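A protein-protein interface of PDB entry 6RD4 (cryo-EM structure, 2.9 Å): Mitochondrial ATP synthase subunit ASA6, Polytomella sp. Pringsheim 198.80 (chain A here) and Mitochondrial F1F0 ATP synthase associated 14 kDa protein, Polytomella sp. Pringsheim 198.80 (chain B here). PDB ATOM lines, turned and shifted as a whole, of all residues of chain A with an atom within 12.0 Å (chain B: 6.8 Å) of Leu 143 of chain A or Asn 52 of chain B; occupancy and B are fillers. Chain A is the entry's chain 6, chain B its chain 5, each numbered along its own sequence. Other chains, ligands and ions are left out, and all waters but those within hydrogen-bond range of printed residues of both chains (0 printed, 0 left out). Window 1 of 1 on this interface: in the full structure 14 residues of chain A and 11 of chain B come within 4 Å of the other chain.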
ATOM      1  N   VAL A  32      42.530 -17.151 -21.818  1.00  0.00           N
ATOM      2  CA  VAL A  32      41.488 -17.503 -20.872  1.00  0.00           C
ATOM      3  C   VAL A  32      41.046 -18.936 -21.088  1.00  0.00           C
ATOM      4  O   VAL A  32      40.846 -19.678 -20.129  1.00  0.00           O
ATOM      5  CB  VAL A  32      40.337 -16.501 -20.983  1.00  0.00           C
ATOM      6  CG1 VAL A  32      39.245 -16.877 -20.084  1.00  0.00           C
ATOM      7  CG2 VAL A  32      40.834 -15.180 -20.573  1.00  0.00           C
ATOM      8  N   THR A 139      41.047   8.751 -18.987  1.00  0.00           N
ATOM      9  CA  THR A 139      41.272   7.326 -18.856  1.00  0.00           C
ATOM     10  C   THR A 139      40.235   6.632 -19.725  1.00  0.00           C
ATOM     11  O   THR A 139      39.204   7.223 -20.041  1.00  0.00           O
ATOM     12  CB  THR A 139      41.121   6.912 -17.394  1.00  0.00           C
ATOM     13  OG1 THR A 139      41.770   7.882 -16.577  1.00  0.00           O
ATOM     14  CG2 THR A 139      41.801   5.580 -17.113  1.00  0.00           C
ATOM     15  N   LEU A 140      40.509   5.395 -20.135  1.00  0.00           N
ATOM     16  CA  LEU A 140      39.495   4.617 -20.823  1.00  0.00           C
ATOM     17  C   LEU A 140      38.293   4.358 -19.936  1.00  0.00           C
ATOM     18  O   LEU A 140      38.399   4.283 -18.716  1.00  0.00           O
ATOM     19  CB  LEU A 140      40.039   3.290 -21.293  1.00  0.00           C
ATOM     20  CG  LEU A 140      40.603   3.274 -22.677  1.00  0.00           C
ATOM     21  CD1 LEU A 140      40.976   1.906 -22.881  1.00  0.00           C
ATOM     22  CD2 LEU A 140      39.521   3.613 -23.612  1.00  0.00           C
ATOM     23  N   ASN A 141      37.142   4.188 -20.563  1.00  0.00           N
ATOM     24  CA  ASN A 141      35.908   4.350 -19.841  1.00  0.00           C
ATOM     25  C   ASN A 141      34.940   3.184 -19.890  1.00  0.00           C
ATOM     26  O   ASN A 141      34.001   3.178 -19.096  1.00  0.00           O
ATOM     27  CB  ASN A 141      35.170   5.587 -20.337  1.00  0.00           C
ATOM     28  CG  ASN A 141      34.348   6.218 -19.269  1.00  0.00           C
ATOM     29  OD1 ASN A 141      34.631   6.054 -18.089  1.00  0.00           O
ATOM     30  ND2 ASN A 141      33.307   6.935 -19.666  1.00  0.00           N
ATOM     31  N   GLY A 142      35.101   2.210 -20.756  1.00  0.00           N
ATOM     32  CA  GLY A 142      34.111   1.156 -20.810  1.00  0.00           C
ATOM     33  C   GLY A 142      34.264   0.127 -19.720  1.00  0.00           C
ATOM     34  O   GLY A 142      35.080   0.268 -18.818  1.00  0.00           O
ATOM     35  N   LEU A 143      33.397  -0.883 -19.779  1.00  0.00           N
ATOM     36  CA  LEU A 143      33.522  -2.189 -19.119  1.00  0.00           C
ATOM     37  C   LEU A 143      33.757  -2.079 -17.610  1.00  0.00           C
ATOM     38  O   LEU A 143      34.877  -2.133 -17.124  1.00  0.00           O
ATOM     39  CB  LEU A 143      34.574  -3.064 -19.772  1.00  0.00           C
ATOM     40  CG  LEU A 143      34.239  -4.491 -19.361  1.00  0.00           C
ATOM     41  CD1 LEU A 143      33.056  -4.948 -20.067  1.00  0.00           C
ATOM     42  CD2 LEU A 143      35.316  -5.419 -19.644  1.00  0.00           C
ATOM     43  N   LYS A 144      32.671  -1.805 -16.890  1.00  0.00           N
ATOM     44  CA  LYS A 144      32.742  -1.426 -15.489  1.00  0.00           C
ATOM     45  C   LYS A 144      32.597  -2.582 -14.513  1.00  0.00           C
ATOM     46  O   LYS A 144      31.983  -2.387 -13.455  1.00  0.00           O
ATOM     47  CB  LYS A 144      31.712  -0.346 -15.178  1.00  0.00           C
ATOM     48  CG  LYS A 144      32.044   0.946 -15.795  1.00  0.00           C
ATOM     49  CD  LYS A 144      33.301   1.449 -15.185  1.00  0.00           C
ATOM     50  CE  LYS A 144      33.782   2.679 -15.888  1.00  0.00           C
ATOM     51  NZ  LYS A 144      35.117   3.097 -15.400  1.00  0.00           N
ATOM     52  N   THR A 145      33.062  -3.786 -14.855  1.00  0.00           N
ATOM     53  CA  THR A 145      33.412  -4.869 -13.920  1.00  0.00           C
ATOM     54  C   THR A 145      32.233  -5.530 -13.209  1.00  0.00           C
ATOM     55  O   THR A 145      32.207  -6.753 -13.088  1.00  0.00           O
ATOM     56  CB  THR A 145      34.403  -4.349 -12.858  1.00  0.00           C
ATOM     57  OG1 THR A 145      35.653  -4.029 -13.471  1.00  0.00           O
ATOM     58  CG2 THR A 145      34.682  -5.367 -11.770  1.00  0.00           C
ATOM     59  N   PHE A 146      31.174  -4.794 -12.908  1.00  0.00           N
ATOM     60  CA  PHE A 146      29.960  -5.389 -12.381  1.00  0.00           C
ATOM     61  C   PHE A 146      29.056  -5.896 -13.467  1.00  0.00           C
ATOM     62  O   PHE A 146      28.116  -6.631 -13.172  1.00  0.00           O
ATOM     63  CB  PHE A 146      29.184  -4.380 -11.544  1.00  0.00           C
ATOM     64  CG  PHE A 146      29.254  -4.612 -10.076  1.00  0.00           C
ATOM     65  CD1 PHE A 146      28.254  -5.303  -9.446  1.00  0.00           C
ATOM     66  CD2 PHE A 146      30.312  -4.163  -9.331  1.00  0.00           C
ATOM     67  CE1 PHE A 146      28.293  -5.509  -8.098  1.00  0.00           C
ATOM     68  CE2 PHE A 146      30.357  -4.380  -7.989  1.00  0.00           C
ATOM     69  CZ  PHE A 146      29.351  -5.052  -7.374  1.00  0.00           C
ATOM     70  N   SER A 147      29.304  -5.504 -14.703  1.00  0.00           N
ATOM     71  CA  SER A 147      28.516  -6.001 -15.804  1.00  0.00           C
ATOM     72  C   SER A 147      29.079  -7.280 -16.376  1.00  0.00           C
ATOM     73  O   SER A 147      28.338  -8.047 -16.982  1.00  0.00           O
ATOM     74  CB  SER A 147      28.417  -4.943 -16.886  1.00  0.00           C
ATOM     75  OG  SER A 147      29.694  -4.634 -17.367  1.00  0.00           O
ATOM     76  N   SER A 148      30.358  -7.547 -16.174  1.00  0.00           N
ATOM     77  CA  SER A 148      31.010  -8.679 -16.808  1.00  0.00           C
ATOM     78  C   SER A 148      31.456  -9.732 -15.809  1.00  0.00           C
ATOM     79  O   SER A 148      32.442 -10.420 -16.062  1.00  0.00           O
ATOM     80  CB  SER A 148      32.203  -8.204 -17.615  1.00  0.00           C
ATOM     81  OG  SER A 148      33.048  -7.438 -16.791  1.00  0.00           O
ATOM     82  N   ILE A 149      30.770  -9.878 -14.685  1.00  0.00           N
ATOM     83  CA  ILE A 149      31.124 -10.941 -13.762  1.00  0.00           C
ATOM     84  C   ILE A 149      30.605 -12.267 -14.294  1.00  0.00           C
ATOM     85  O   ILE A 149      29.729 -12.323 -15.149  1.00  0.00           O
ATOM     86  CB  ILE A 149      30.567 -10.688 -12.365  1.00  0.00           C
ATOM     87  CG1 ILE A 149      29.090 -10.554 -12.508  1.00  0.00           C
ATOM     88  CG2 ILE A 149      31.121  -9.473 -11.732  1.00  0.00           C
ATOM     89  CD1 ILE A 149      28.447 -10.868 -11.325  1.00  0.00           C
ATOM     90  N   SER A 150      31.151 -13.353 -13.763  1.00  0.00           N
ATOM     91  CA  SER A 150      30.678 -14.695 -14.089  1.00  0.00           C
ATOM     92  C   SER A 150      30.565 -15.461 -12.773  1.00  0.00           C
ATOM     93  O   SER A 150      31.492 -16.154 -12.361  1.00  0.00           O
ATOM     94  CB  SER A 150      31.617 -15.386 -15.058  1.00  0.00           C
ATOM     95  OG  SER A 150      31.760 -14.666 -16.252  1.00  0.00           O
ATOM     96  N   TRP B  44      34.956   3.703 -26.972  1.00  0.00           N
ATOM     97  CA  TRP B  44      34.768   3.148 -25.651  1.00  0.00           C
ATOM     98  C   TRP B  44      34.137   4.150 -24.715  1.00  0.00           C
ATOM     99  O   TRP B  44      33.456   3.770 -23.774  1.00  0.00           O
ATOM    100  CB  TRP B  44      36.092   2.683 -25.091  1.00  0.00           C
ATOM    101  CG  TRP B  44      36.395   1.263 -25.300  1.00  0.00           C
ATOM    102  CD1 TRP B  44      37.437   0.762 -25.974  1.00  0.00           C
ATOM    103  CD2 TRP B  44      35.665   0.150 -24.804  1.00  0.00           C
ATOM    104  NE1 TRP B  44      37.416  -0.594 -25.943  1.00  0.00           N
ATOM    105  CE2 TRP B  44      36.325  -0.993 -25.228  1.00  0.00           C
ATOM    106  CE3 TRP B  44      34.494   0.011 -24.066  1.00  0.00           C
ATOM    107  CZ2 TRP B  44      35.868  -2.249 -24.929  1.00  0.00           C
ATOM    108  CZ3 TRP B  44      34.071  -1.205 -23.756  1.00  0.00           C
ATOM    109  CH2 TRP B  44      34.741  -2.333 -24.187  1.00  0.00           C
ATOM    110  N   ALA B  47      30.341   4.355 -26.038  1.00  0.00           N
ATOM    111  CA  ALA B  47      29.537   3.170 -25.844  1.00  0.00           C
ATOM    112  C   ALA B  47      29.426   2.742 -24.411  1.00  0.00           C
ATOM    113  O   ALA B  47      28.558   1.925 -24.134  1.00  0.00           O
ATOM    114  CB  ALA B  47      30.102   1.991 -26.599  1.00  0.00           C
ATOM    115  N   ALA B  48      30.245   3.290 -23.505  1.00  0.00           N
ATOM    116  CA  ALA B  48      30.432   2.744 -22.163  1.00  0.00           C
ATOM    117  C   ALA B  48      29.152   2.636 -21.376  1.00  0.00           C
ATOM    118  O   ALA B  48      29.013   1.747 -20.539  1.00  0.00           O
ATOM    119  CB  ALA B  48      31.374   3.615 -21.362  1.00  0.00           C
ATOM    120  N   LYS B  49      28.213   3.534 -21.610  1.00  0.00           N
ATOM    121  CA  LYS B  49      26.967   3.490 -20.878  1.00  0.00           C
ATOM    122  C   LYS B  49      26.016   2.474 -21.472  1.00  0.00           C
ATOM    123  O   LYS B  49      25.294   1.803 -20.740  1.00  0.00           O
ATOM    124  CB  LYS B  49      26.340   4.869 -20.871  1.00  0.00           C
ATOM    125  CG  LYS B  49      25.292   5.035 -19.843  1.00  0.00           C
ATOM    126  CD  LYS B  49      24.437   6.226 -20.143  1.00  0.00           C
ATOM    127  CE  LYS B  49      23.235   6.237 -19.238  1.00  0.00           C
ATOM    128  NZ  LYS B  49      22.593   4.897 -19.236  1.00  0.00           N
ATOM    129  N   ARG B  50      25.997   2.352 -22.788  1.00  0.00           N
ATOM    130  CA  ARG B  50      25.138   1.397 -23.461  1.00  0.00           C
ATOM    131  C   ARG B  50      25.775   0.039 -23.610  1.00  0.00           C
ATOM    132  O   ARG B  50      25.065  -0.928 -23.853  1.00  0.00           O
ATOM    133  CB  ARG B  50      24.766   1.911 -24.839  1.00  0.00           C
ATOM    134  CG  ARG B  50      23.892   3.105 -24.790  1.00  0.00           C
ATOM    135  CD  ARG B  50      23.686   3.694 -26.140  1.00  0.00           C
ATOM    136  NE  ARG B  50      23.466   2.688 -27.159  1.00  0.00           N
ATOM    137  CZ  ARG B  50      22.784   2.921 -28.270  1.00  0.00           C
ATOM    138  NH1 ARG B  50      22.630   1.961 -29.167  1.00  0.00           N
ATOM    139  NH2 ARG B  50      22.256   4.121 -28.479  1.00  0.00           N
ATOM    140  N   TYR B  51      27.096  -0.046 -23.540  1.00  0.00           N
ATOM    141  CA  TYR B  51      27.769  -1.333 -23.559  1.00  0.00           C
ATOM    142  C   TYR B  51      27.536  -2.059 -22.259  1.00  0.00           C
ATOM    143  O   TYR B  51      27.228  -3.246 -22.242  1.00  0.00           O
ATOM    144  CB  TYR B  51      29.256  -1.114 -23.768  1.00  0.00           C
ATOM    145  CG  TYR B  51      30.086  -2.308 -23.986  1.00  0.00           C
ATOM    146  CD1 TYR B  51      30.272  -2.795 -25.250  1.00  0.00           C
ATOM    147  CD2 TYR B  51      30.737  -2.909 -22.943  1.00  0.00           C
ATOM    148  CE1 TYR B  51      31.037  -3.870 -25.459  1.00  0.00           C
ATOM    149  CE2 TYR B  51      31.500  -3.980 -23.145  1.00  0.00           C
ATOM    150  CZ  TYR B  51      31.651  -4.459 -24.399  1.00  0.00           C
ATOM    151  OH  TYR B  51      32.438  -5.544 -24.585  1.00  0.00           O
ATOM    152  N   ASN B  52      27.694  -1.351 -21.155  1.00  0.00           N
ATOM    153  CA  ASN B  52      27.579  -1.947 -19.846  1.00  0.00           C
ATOM    154  C   ASN B  52      26.150  -2.263 -19.501  1.00  0.00           C
ATOM    155  O   ASN B  52      25.897  -3.204 -18.764  1.00  0.00           O
ATOM    156  CB  ASN B  52      28.147  -1.007 -18.815  1.00  0.00           C
ATOM    157  CG  ASN B  52      29.604  -0.917 -18.892  1.00  0.00           C
ATOM    158  OD1 ASN B  52      30.262  -1.905 -19.086  1.00  0.00           O
ATOM    159  ND2 ASN B  52      30.129   0.269 -18.756  1.00  0.00           N
ATOM    160  N   GLU B  53      25.208  -1.486 -20.000  1.00  0.00           N
ATOM    161  CA  GLU B  53      23.810  -1.799 -19.775  1.00  0.00           C
ATOM    162  C   GLU B  53      23.365  -2.954 -20.645  1.00  0.00           C
ATOM    163  O   GLU B  53      22.527  -3.746 -20.232  1.00  0.00           O
ATOM    164  CB  GLU B  53      22.965  -0.564 -20.030  1.00  0.00           C
ATOM    165  CG  GLU B  53      21.500  -0.717 -19.718  1.00  0.00           C
ATOM    166  CD  GLU B  53      21.220  -1.069 -18.273  1.00  0.00           C
ATOM    167  OE1 GLU B  53      21.570  -0.271 -17.384  1.00  0.00           O
ATOM    168  OE2 GLU B  53      20.640  -2.142 -18.028  1.00  0.00           O
ATOM    169  N   LYS B  54      23.920  -3.089 -21.839  1.00  0.00           N
ATOM    170  CA  LYS B  54      23.603  -4.246 -22.661  1.00  0.00           C
ATOM    171  C   LYS B  54      24.219  -5.507 -22.102  1.00  0.00           C
ATOM    172  O   LYS B  54      23.651  -6.587 -22.227  1.00  0.00           O
ATOM    173  CB  LYS B  54      24.081  -4.023 -24.086  1.00  0.00           C
ATOM    174  CG  LYS B  54      23.620  -5.047 -25.057  1.00  0.00           C
ATOM    175  CD  LYS B  54      24.119  -4.750 -26.417  1.00  0.00           C
ATOM    176  CE  LYS B  54      23.595  -5.756 -27.390  1.00  0.00           C
ATOM    177  NZ  LYS B  54      24.141  -5.565 -28.748  1.00  0.00           N
ATOM    178  N   LEU B  55      25.371  -5.388 -21.481  1.00  0.00           N
ATOM    179  CA  LEU B  55      26.036  -6.527 -20.885  1.00  0.00           C
ATOM    180  C   LEU B  55      25.404  -6.909 -19.565  1.00  0.00           C
ATOM    181  O   LEU B  55      25.389  -8.085 -19.216  1.00  0.00           O
ATOM    182  CB  LEU B  55      27.506  -6.186 -20.709  1.00  0.00           C
ATOM    183  CG  LEU B  55      28.529  -7.251 -20.422  1.00  0.00           C
ATOM    184  CD1 LEU B  55      28.353  -8.342 -21.355  1.00  0.00           C
ATOM    185  CD2 LEU B  55      29.828  -6.639 -20.641  1.00  0.00           C
ATOM    186  N   PHE B  56      24.894  -5.932 -18.825  1.00  0.00           N
ATOM    187  CA  PHE B  56      24.145  -6.193 -17.606  1.00  0.00           C
ATOM    188  C   PHE B  56      22.884  -6.972 -17.899  1.00  0.00           C
ATOM    189  O   PHE B  56      22.532  -7.892 -17.163  1.00  0.00           O
ATOM    190  CB  PHE B  56      23.782  -4.877 -16.955  1.00  0.00           C
ATOM    191  CG  PHE B  56      23.298  -4.993 -15.569  1.00  0.00           C
ATOM    192  CD1 PHE B  56      24.167  -5.274 -14.559  1.00  0.00           C
ATOM    193  CD2 PHE B  56      21.981  -4.769 -15.265  1.00  0.00           C
ATOM    194  CE1 PHE B  56      23.729  -5.361 -13.283  1.00  0.00           C
ATOM    195  CE2 PHE B  56      21.550  -4.858 -13.984  1.00  0.00           C
ATOM    196  CZ  PHE B  56      22.425  -5.149 -12.998  1.00  0.00           C
ATOM    197  N   LYS B  57      22.205  -6.641 -18.988  1.00  0.00           N
ATOM    198  CA  LYS B  57      20.999  -7.358 -19.346  1.00  0.00           C
ATOM    199  C   LYS B  57      21.282  -8.731 -19.906  1.00  0.00           C
ATOM    200  O   LYS B  57      20.363  -9.535 -20.017  1.00  0.00           O
ATOM    201  CB  LYS B  57      20.205  -6.567 -20.363  1.00  0.00           C
ATOM    202  CG  LYS B  57      19.667  -5.273 -19.851  1.00  0.00           C
ATOM    203  CD  LYS B  57      19.049  -4.495 -20.986  1.00  0.00           C
ATOM    204  CE  LYS B  57      18.783  -3.069 -20.582  1.00  0.00           C
ATOM    205  NZ  LYS B  57      18.459  -2.191 -21.732  1.00  0.00           N
ATOM    206  N   TYR B  62      23.435 -12.834 -12.081  1.00  0.00           N
ATOM    207  CA  TYR B  62      23.016 -12.120 -10.883  1.00  0.00           C
ATOM    208  C   TYR B  62      21.888 -12.802 -10.147  1.00  0.00           C
ATOM    209  O   TYR B  62      21.882 -12.826  -8.919  1.00  0.00           O
ATOM    210  CB  TYR B  62      22.568 -10.714 -11.232  1.00  0.00           C
ATOM    211  CG  TYR B  62      23.578  -9.938 -11.987  1.00  0.00           C
ATOM    212  CD1 TYR B  62      24.747  -9.549 -11.388  1.00  0.00           C
ATOM    213  CD2 TYR B  62      23.348  -9.568 -13.281  1.00  0.00           C
ATOM    214  CE1 TYR B  62      25.661  -8.838 -12.065  1.00  0.00           C
ATOM    215  CE2 TYR B  62      24.259  -8.859 -13.962  1.00  0.00           C
ATOM    216  CZ  TYR B  62      25.416  -8.504 -13.351  1.00  0.00           C
ATOM    217  OH  TYR B  62      26.340  -7.781 -14.030  1.00  0.00           O
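OD1 of Asn 52 of chain B sits close to N of Leu 143 of chain A, at 3.4 Å. OD1 of Asn 52 of chain B lies within hydrogen-bond range of N of Lys 144 of chain A, 3.3 Å away. The side-chain amide oxygen of Asn 52 of chain B sits at hydrogen-bond distance from the side-chain hydroxyl of Ser 147 of chain A (3.3 Å). The side-chain hydroxyl (OH) of Tyr 62 of chain B lies close to the backbone carbonyl oxygen (O) of Phe 146 of chain A, at 2.3 Å.
The side-chain amide nitrogen of Asn 52 of chain B is in hydrogen-bond range of the backbone carbonyl oxygen of Ala 48 of chain B (2.6 Å).
Among the printed residues, merely in contact across the chains: Leu 140 of chain A with Trp 44 of chain B, Asn 141 of chain A with Ala 48 of chain B, Gly 142 of chain A with Trp 44 of chain B, Gly 142 of chain A with Ala 48 of chain B, Leu 143 of chain A with Tyr 51 of chain B, Leu 143 of chain A with Leu 55 of chain B, Ser 147 of chain A with Leu 55 of chain B, Ser 147 of chain A with Tyr 62 of chain B and Ile 149 of chain A with Tyr 62 of chain B.
Of the printed residues of chain B, Asn 141 of chain A touches Ala 48. Printed residues of chain B within 4 Å of Leu 143 of chain A: Tyr 51 (3.6 Å), Asn 52 (3.3 Å) and Leu 55 (3.7 Å). Of the printed residues of chain A, Trp 44 of chain B touches Leu 140 and Gly 142. Asn 52 of chain B touches just these residues of chain A: Leu 143 (3.3 Å), Lys 144 (3.3 Å) and Ser 147 (3.3 Å). No residue of chain A comes within 4 Å of Glu 53 of chain B. Leu 55 of chain B touches just these residues of chain A: Leu 143 and Ser 147. The nearest residue of chain B that does not touch Leu 143 of chain A is Trp 44 of chain B (4.05 Å). The nearest residue of chain A that does not touch Asn 52 of chain B is Gly 142 of chain A (4.2 Å).
Of the 13 printed residues of chain A, 8 touch a printed residue of chain B. Hydrophobic or aromatic side chains of chain A within 4 Å of the printed part of chain B: Leu 140, Leu 143 and Ile 149. Among the printed residues, no Asp or Glu carboxylate lies within 4 Å of a Lys or Arg side-chain nitrogen of the other chain.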
